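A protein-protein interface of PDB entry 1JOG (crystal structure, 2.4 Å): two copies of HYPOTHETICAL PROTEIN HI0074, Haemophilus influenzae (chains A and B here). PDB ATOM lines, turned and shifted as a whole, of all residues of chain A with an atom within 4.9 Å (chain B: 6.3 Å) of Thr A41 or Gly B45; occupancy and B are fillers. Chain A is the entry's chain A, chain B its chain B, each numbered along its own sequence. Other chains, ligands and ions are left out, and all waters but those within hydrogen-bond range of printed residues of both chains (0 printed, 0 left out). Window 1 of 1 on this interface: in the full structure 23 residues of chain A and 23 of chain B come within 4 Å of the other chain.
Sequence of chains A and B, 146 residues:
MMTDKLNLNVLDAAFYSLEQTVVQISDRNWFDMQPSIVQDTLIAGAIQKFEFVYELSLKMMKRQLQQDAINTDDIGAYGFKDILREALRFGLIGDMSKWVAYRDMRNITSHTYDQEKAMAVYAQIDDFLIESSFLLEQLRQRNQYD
The side-chain carboxylate of Asp A40 lies within salt-bridge range of the side-chain amino group of Lys B49 (3.4 Å). The side-chain hydroxyl (OG1) of Thr A41 is in hydrogen-bond range of the side-chain hydroxyl (OG1) of Thr B21 (2.9 Å). The side-chain hydroxyl (OG1) of Thr A41 lies within hydrogen-bond range of the side-chain amino group (NZ) of Lys B49 (3.3 Å).
The side-chain amino group (NZ) of Lys B49 sits at hydrogen-bond distance from the side-chain hydroxyl (OG) of Ser B17. OG1 of Thr B21 sits at hydrogen-bond distance from NZ of Lys B49 (2.5 Å). OD2 of Asp B40 lies within hydrogen-bond range of OG1 of Thr B41 (3.3 Å). OG1 of Thr A41 sits at hydrogen-bond distance from O of Ile A37 (2.9 Å). The backbone carbonyl oxygen (O) of Ser B17 is in hydrogen-bond range of the side-chain hydroxyl (OG1) of Thr B21 (2.7 Å).
Ile A37 touches Ser B17 (CD1 to O, 3.7 Å). OG1 of Thr B21 touches CD1 of Ile A37, at 3.5 Å. Lys B49 touches Ile A37 (NZ to CD1, 3.2 Å). Ser B17 touches Asp A40. CD2 of Leu B42 touches CG2 of Thr A41 (3.3 Å). Thr A41 touches Gly B45 (O to CA, 3.4 Å). CD2 of Leu A42 touches CG2 of Thr B41, 3.0 Å away. Thr B41 touches Gly A45 (O to CA, 3.7 Å). Gly A45 touches Ala B44. Gly B45 touches Gly A45.
Of the printed residues of chain B, Ile A37 touches Ser B17 (3.7 Å), Thr B21 (3.5 Å) and Lys B49 (3.2 Å). Of the printed residues of chain B, Asp A40 touches Ser B17 and Lys B49. Thr A41 touches just these residues of chain B: Thr B21, Leu B42, Gly B45 and Lys B49. Ile A43 touches none of the printed residues of chain B. Ile B25 touches none of the printed residues of chain A. Of the printed residues of chain A, Leu B42 touches Thr A41 (3.3 Å). Gly B45 touches three residues of chain A.
Of the 9 printed residues of chain A, 6 touch a printed residue of chain B. Hydrophobic or aromatic side chains of chain A within 4 Å of the printed part of chain B: Ile A37, Leu A42 and Ala A44. Of the 15 printed residues of chain B, 7 touch a printed residue of chain A. Hydrophobic or aromatic side chains of chain B within 4 Å of the printed part of chain A: Leu B42 and Ala B44.
Thr A41 touches Leu B42, and with the chains exchanged Leu A42 touches Thr B41. Thr A41 touches Gly B45, and with the chains exchanged Gly A45 touches Thr B41. Ala A44 touches Gly B45, and with the chains exchanged Gly A45 touches Ala B44. Gly A45 touches its own counterpart, Gly B45. 6 positions are printed for both chains.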
ATOM      1  N   ILE A  37      -6.952  21.840   4.330  1.00  0.00           N
ATOM      2  CA  ILE A  37      -8.260  21.849   3.743  1.00  0.00           C
ATOM      3  C   ILE A  37      -8.209  22.461   2.339  1.00  0.00           C
ATOM      4  O   ILE A  37      -9.044  22.119   1.505  1.00  0.00           O
ATOM      5  CB  ILE A  37      -9.295  22.559   4.692  1.00  0.00           C
ATOM      6  CG1 ILE A  37     -10.734  22.265   4.269  1.00  0.00           C
ATOM      7  CG2 ILE A  37      -9.205  24.058   4.573  1.00  0.00           C
ATOM      8  CD1 ILE A  37     -11.116  20.822   4.321  1.00  0.00           C
ATOM      9  N   VAL A  38      -7.235  23.349   2.083  1.00  0.00           N
ATOM     10  CA  VAL A  38      -7.069  23.971   0.754  1.00  0.00           C
ATOM     11  C   VAL A  38      -6.562  22.861  -0.185  1.00  0.00           C
ATOM     12  O   VAL A  38      -7.098  22.662  -1.267  1.00  0.00           O
ATOM     13  CB  VAL A  38      -6.094  25.169   0.818  1.00  0.00           C
ATOM     14  CG1 VAL A  38      -5.658  25.637  -0.634  1.00  0.00           C
ATOM     15  CG2 VAL A  38      -6.784  26.323   1.566  1.00  0.00           C
ATOM     16  N   GLN A  39      -5.586  22.076   0.255  1.00  0.00           N
ATOM     17  CA  GLN A  39      -5.079  21.042  -0.607  1.00  0.00           C
ATOM     18  C   GLN A  39      -6.155  20.109  -1.073  1.00  0.00           C
ATOM     19  O   GLN A  39      -6.212  19.830  -2.241  1.00  0.00           O
ATOM     20  CB  GLN A  39      -3.991  20.191   0.055  1.00  0.00           C
ATOM     21  CG  GLN A  39      -2.663  20.914   0.223  1.00  0.00           C
ATOM     22  CD  GLN A  39      -1.585  20.043   0.854  1.00  0.00           C
ATOM     23  OE1 GLN A  39      -1.809  19.457   1.914  1.00  0.00           O
ATOM     24  NE2 GLN A  39      -0.451  19.929   0.201  1.00  0.00           N
ATOM     25  N   ASP A  40      -7.029  19.621  -0.191  1.00  0.00           N
ATOM     26  CA  ASP A  40      -8.009  18.655  -0.684  1.00  0.00           C
ATOM     27  C   ASP A  40      -9.262  19.247  -1.314  1.00  0.00           C
ATOM     28  O   ASP A  40      -9.978  18.551  -2.068  1.00  0.00           O
ATOM     29  CB  ASP A  40      -8.382  17.668   0.404  1.00  0.00           C
ATOM     30  CG  ASP A  40      -9.368  18.219   1.402  1.00  0.00           C
ATOM     31  OD1 ASP A  40      -9.164  19.331   1.946  1.00  0.00           O
ATOM     32  OD2 ASP A  40     -10.358  17.506   1.655  1.00  0.00           O
ATOM     33  N   THR A  41      -9.551  20.502  -1.003  1.00  0.00           N
ATOM     34  CA  THR A  41     -10.712  21.098  -1.612  1.00  0.00           C
ATOM     35  C   THR A  41     -10.338  21.231  -3.080  1.00  0.00           C
ATOM     36  O   THR A  41     -11.160  21.017  -3.949  1.00  0.00           O
ATOM     37  CB  THR A  41     -11.010  22.442  -1.033  1.00  0.00           C
ATOM     38  OG1 THR A  41     -11.619  22.248   0.262  1.00  0.00           O
ATOM     39  CG2 THR A  41     -12.018  23.282  -2.003  1.00  0.00           C
ATOM     40  N   LEU A  42      -9.063  21.523  -3.323  1.00  0.00           N
ATOM     41  CA  LEU A  42      -8.530  21.691  -4.658  1.00  0.00           C
ATOM     42  C   LEU A  42      -8.548  20.418  -5.463  1.00  0.00           C
ATOM     43  O   LEU A  42      -8.738  20.459  -6.684  1.00  0.00           O
ATOM     44  CB  LEU A  42      -7.108  22.197  -4.624  1.00  0.00           C
ATOM     45  CG  LEU A  42      -6.978  23.703  -4.517  1.00  0.00           C
ATOM     46  CD1 LEU A  42      -5.503  24.077  -4.342  1.00  0.00           C
ATOM     47  CD2 LEU A  42      -7.644  24.338  -5.773  1.00  0.00           C
ATOM     48  N   ILE A  43      -8.309  19.307  -4.796  1.00  0.00           N
ATOM     49  CA  ILE A  43      -8.365  18.019  -5.478  1.00  0.00           C
ATOM     50  C   ILE A  43      -9.822  17.695  -5.689  1.00  0.00           C
ATOM     51  O   ILE A  43     -10.186  17.152  -6.720  1.00  0.00           O
ATOM     52  CB  ILE A  43      -7.679  16.905  -4.615  1.00  0.00           C
ATOM     53  CG1 ILE A  43      -6.159  17.008  -4.791  1.00  0.00           C
ATOM     54  CG2 ILE A  43      -8.128  15.499  -5.065  1.00  0.00           C
ATOM     55  CD1 ILE A  43      -5.457  15.851  -4.108  1.00  0.00           C
ATOM     56  N   ALA A  44     -10.660  17.990  -4.688  1.00  0.00           N
ATOM     57  CA  ALA A  44     -12.124  17.801  -4.801  1.00  0.00           C
ATOM     58  C   ALA A  44     -12.581  18.584  -6.066  1.00  0.00           C
ATOM     59  O   ALA A  44     -13.252  18.059  -6.921  1.00  0.00           O
ATOM     60  CB  ALA A  44     -12.817  18.401  -3.611  1.00  0.00           C
ATOM     61  N   GLY A  45     -12.136  19.835  -6.181  1.00  0.00           N
ATOM     62  CA  GLY A  45     -12.515  20.700  -7.293  1.00  0.00           C
ATOM     63  C   GLY A  45     -12.053  20.253  -8.661  1.00  0.00           C
ATOM     64  O   GLY A  45     -12.803  20.382  -9.612  1.00  0.00           O
ATOM     65  N   SER B  17     -15.622  18.313   6.726  1.00  0.00           N
ATOM     66  CA  SER B  17     -14.777  18.726   5.623  1.00  0.00           C
ATOM     67  C   SER B  17     -15.489  19.822   4.868  1.00  0.00           C
ATOM     68  O   SER B  17     -14.782  20.728   4.385  1.00  0.00           O
ATOM     69  CB  SER B  17     -14.545  17.525   4.664  1.00  0.00           C
ATOM     70  OG  SER B  17     -13.701  17.866   3.576  1.00  0.00           O
ATOM     71  N   LEU B  18     -16.846  19.730   4.712  1.00  0.00           N
ATOM     72  CA  LEU B  18     -17.602  20.780   3.954  1.00  0.00           C
ATOM     73  C   LEU B  18     -17.563  22.059   4.792  1.00  0.00           C
ATOM     74  O   LEU B  18     -17.288  23.153   4.305  1.00  0.00           O
ATOM     75  CB  LEU B  18     -19.083  20.419   3.707  1.00  0.00           C
ATOM     76  CG  LEU B  18     -19.677  20.985   2.405  1.00  0.00           C
ATOM     77  CD1 LEU B  18     -21.170  21.017   2.487  1.00  0.00           C
ATOM     78  CD2 LEU B  18     -19.183  22.334   2.083  1.00  0.00           C
ATOM     79  N   THR B  21     -14.300  23.565   4.752  1.00  0.00           N
ATOM     80  CA  THR B  21     -14.051  24.201   3.466  1.00  0.00           C
ATOM     81  C   THR B  21     -14.722  25.553   3.410  1.00  0.00           C
ATOM     82  O   THR B  21     -14.061  26.489   3.027  1.00  0.00           O
ATOM     83  CB  THR B  21     -14.504  23.262   2.320  1.00  0.00           C
ATOM     84  OG1 THR B  21     -13.649  22.122   2.309  1.00  0.00           O
ATOM     85  CG2 THR B  21     -14.516  23.933   0.978  1.00  0.00           C
ATOM     86  N   ILE B  25     -12.897  29.409   2.656  1.00  0.00           N
ATOM     87  CA  ILE B  25     -13.401  30.302   1.605  1.00  0.00           C
ATOM     88  C   ILE B  25     -13.993  31.569   2.230  1.00  0.00           C
ATOM     89  O   ILE B  25     -13.931  32.656   1.645  1.00  0.00           O
ATOM     90  CB  ILE B  25     -14.477  29.588   0.763  1.00  0.00           C
ATOM     91  CG1 ILE B  25     -13.752  28.526  -0.030  1.00  0.00           C
ATOM     92  CG2 ILE B  25     -15.343  30.622  -0.093  1.00  0.00           C
ATOM     93  CD1 ILE B  25     -14.597  27.466  -0.707  1.00  0.00           C
ATOM     94  N   ASP B  40     -11.742  29.724  -8.101  1.00  0.00           N
ATOM     95  CA  ASP B  40     -12.847  28.940  -8.666  1.00  0.00           C
ATOM     96  C   ASP B  40     -12.723  27.440  -8.419  1.00  0.00           C
ATOM     97  O   ASP B  40     -13.734  26.727  -8.374  1.00  0.00           O
ATOM     98  CB  ASP B  40     -13.097  29.315 -10.114  1.00  0.00           C
ATOM     99  CG  ASP B  40     -12.219  28.577 -11.057  1.00  0.00           C
ATOM    100  OD1 ASP B  40     -11.977  29.110 -12.140  1.00  0.00           O
ATOM    101  OD2 ASP B  40     -11.775  27.469 -10.726  1.00  0.00           O
ATOM    102  N   THR B  41     -11.500  26.951  -8.181  1.00  0.00           N
ATOM    103  CA  THR B  41     -11.345  25.519  -7.908  1.00  0.00           C
ATOM    104  C   THR B  41     -11.901  25.207  -6.515  1.00  0.00           C
ATOM    105  O   THR B  41     -12.647  24.259  -6.320  1.00  0.00           O
ATOM    106  CB  THR B  41      -9.885  25.100  -8.080  1.00  0.00           C
ATOM    107  OG1 THR B  41      -9.440  25.470  -9.397  1.00  0.00           O
ATOM    108  CG2 THR B  41      -9.752  23.650  -7.859  1.00  0.00           C
ATOM    109  N   LEU B  42     -11.616  26.060  -5.549  1.00  0.00           N
ATOM    110  CA  LEU B  42     -12.176  25.863  -4.204  1.00  0.00           C
ATOM    111  C   LEU B  42     -13.707  25.894  -4.322  1.00  0.00           C
ATOM    112  O   LEU B  42     -14.380  25.002  -3.769  1.00  0.00           O
ATOM    113  CB  LEU B  42     -11.662  26.975  -3.232  1.00  0.00           C
ATOM    114  CG  LEU B  42     -10.125  26.876  -3.103  1.00  0.00           C
ATOM    115  CD1 LEU B  42      -9.486  28.141  -2.582  1.00  0.00           C
ATOM    116  CD2 LEU B  42      -9.779  25.712  -2.240  1.00  0.00           C
ATOM    117  N   ILE B  43     -14.287  26.898  -5.005  1.00  0.00           N
ATOM    118  CA  ILE B  43     -15.768  26.855  -5.128  1.00  0.00           C
ATOM    119  C   ILE B  43     -16.271  25.483  -5.632  1.00  0.00           C
ATOM    120  O   ILE B  43     -17.196  24.869  -5.044  1.00  0.00           O
ATOM    121  CB  ILE B  43     -16.364  27.975  -6.123  1.00  0.00           C
ATOM    122  CG1 ILE B  43     -16.303  29.361  -5.487  1.00  0.00           C
ATOM    123  CG2 ILE B  43     -17.885  27.784  -6.331  1.00  0.00           C
ATOM    124  CD1 ILE B  43     -14.970  30.055  -5.578  1.00  0.00           C
ATOM    125  N   ALA B  44     -15.674  25.014  -6.731  1.00  0.00           N
ATOM    126  CA  ALA B  44     -16.032  23.684  -7.348  1.00  0.00           C
ATOM    127  C   ALA B  44     -15.824  22.547  -6.315  1.00  0.00           C
ATOM    128  O   ALA B  44     -16.651  21.649  -6.152  1.00  0.00           O
ATOM    129  CB  ALA B  44     -15.136  23.464  -8.604  1.00  0.00           C
ATOM    130  N   GLY B  45     -14.666  22.577  -5.618  1.00  0.00           N
ATOM    131  CA  GLY B  45     -14.412  21.546  -4.593  1.00  0.00           C
ATOM    132  C   GLY B  45     -15.491  21.673  -3.520  1.00  0.00           C
ATOM    133  O   GLY B  45     -15.956  20.680  -3.013  1.00  0.00           O
ATOM    134  N   ALA B  46     -15.930  22.899  -3.221  1.00  0.00           N
ATOM    135  CA  ALA B  46     -17.003  23.028  -2.214  1.00  0.00           C
ATOM    136  C   ALA B  46     -18.369  22.471  -2.726  1.00  0.00           C
ATOM    137  O   ALA B  46     -19.167  21.867  -1.977  1.00  0.00           O
ATOM    138  CB  ALA B  46     -17.131  24.465  -1.794  1.00  0.00           C
ATOM    139  N   ILE B  47     -18.618  22.681  -4.023  1.00  0.00           N
ATOM    140  CA  ILE B  47     -19.852  22.173  -4.616  1.00  0.00           C
ATOM    141  C   ILE B  47     -19.736  20.662  -4.601  1.00  0.00           C
ATOM    142  O   ILE B  47     -20.693  19.952  -4.192  1.00  0.00           O
ATOM    143  CB  ILE B  47     -20.099  22.729  -6.012  1.00  0.00           C
ATOM    144  CG1 ILE B  47     -20.647  24.161  -5.865  1.00  0.00           C
ATOM    145  CG2 ILE B  47     -21.203  21.905  -6.688  1.00  0.00           C
ATOM    146  CD1 ILE B  47     -20.340  24.975  -7.018  1.00  0.00           C
ATOM    147  N   GLN B  48     -18.566  20.143  -4.944  1.00  0.00           N
ATOM    148  CA  GLN B  48     -18.416  18.680  -4.846  1.00  0.00           C
ATOM    149  C   GLN B  48     -18.639  18.159  -3.407  1.00  0.00           C
ATOM    150  O   GLN B  48     -19.265  17.115  -3.223  1.00  0.00           O
ATOM    151  CB  GLN B  48     -17.039  18.221  -5.275  1.00  0.00           C
ATOM    152  CG  GLN B  48     -16.894  16.729  -5.238  1.00  0.00           C
ATOM    153  CD  GLN B  48     -17.209  16.116  -6.602  1.00  0.00           C
ATOM    154  OE1 GLN B  48     -18.245  16.387  -7.237  1.00  0.00           O
ATOM    155  NE2 GLN B  48     -16.314  15.290  -7.057  1.00  0.00           N
ATOM    156  N   LYS B  49     -18.141  18.894  -2.381  1.00  0.00           N
ATOM    157  CA  LYS B  49     -18.301  18.403  -0.987  1.00  0.00           C
ATOM    158  C   LYS B  49     -19.750  18.521  -0.475  1.00  0.00           C
ATOM    159  O   LYS B  49     -20.167  17.798   0.485  1.00  0.00           O
ATOM    160  CB  LYS B  49     -17.325  19.104  -0.001  1.00  0.00           C
ATOM    161  CG  LYS B  49     -15.833  18.919  -0.264  1.00  0.00           C
ATOM    162  CD  LYS B  49     -15.053  18.947   0.988  1.00  0.00           C
ATOM    163  CE  LYS B  49     -13.643  19.261   0.717  1.00  0.00           C
ATOM    164  NZ  LYS B  49     -12.883  19.736   1.939  1.00  0.00           N
ATOM    165  N   PHE B  50     -20.487  19.445  -1.095  1.00  0.00           N
ATOM    166  CA  PHE B  50     -21.898  19.683  -0.815  1.00  0.00           C
ATOM    167  C   PHE B  50     -22.692  18.430  -1.265  1.00  0.00           C
ATOM    168  O   PHE B  50     -23.573  17.845  -0.535  1.00  0.00           O
ATOM    169  CB  PHE B  50     -22.424  20.919  -1.607  1.00  0.00           C
ATOM    170  CG  PHE B  50     -23.848  20.783  -1.956  1.00  0.00           C
ATOM    171  CD1 PHE B  50     -24.273  20.656  -3.294  1.00  0.00           C
ATOM    172  CD2 PHE B  50     -24.787  20.773  -0.949  1.00  0.00           C
ATOM    173  CE1 PHE B  50     -25.616  20.532  -3.609  1.00  0.00           C
ATOM    174  CE2 PHE B  50     -26.140  20.663  -1.267  1.00  0.00           C
ATOM    175  CZ  PHE B  50     -26.549  20.544  -2.601  1.00  0.00           C
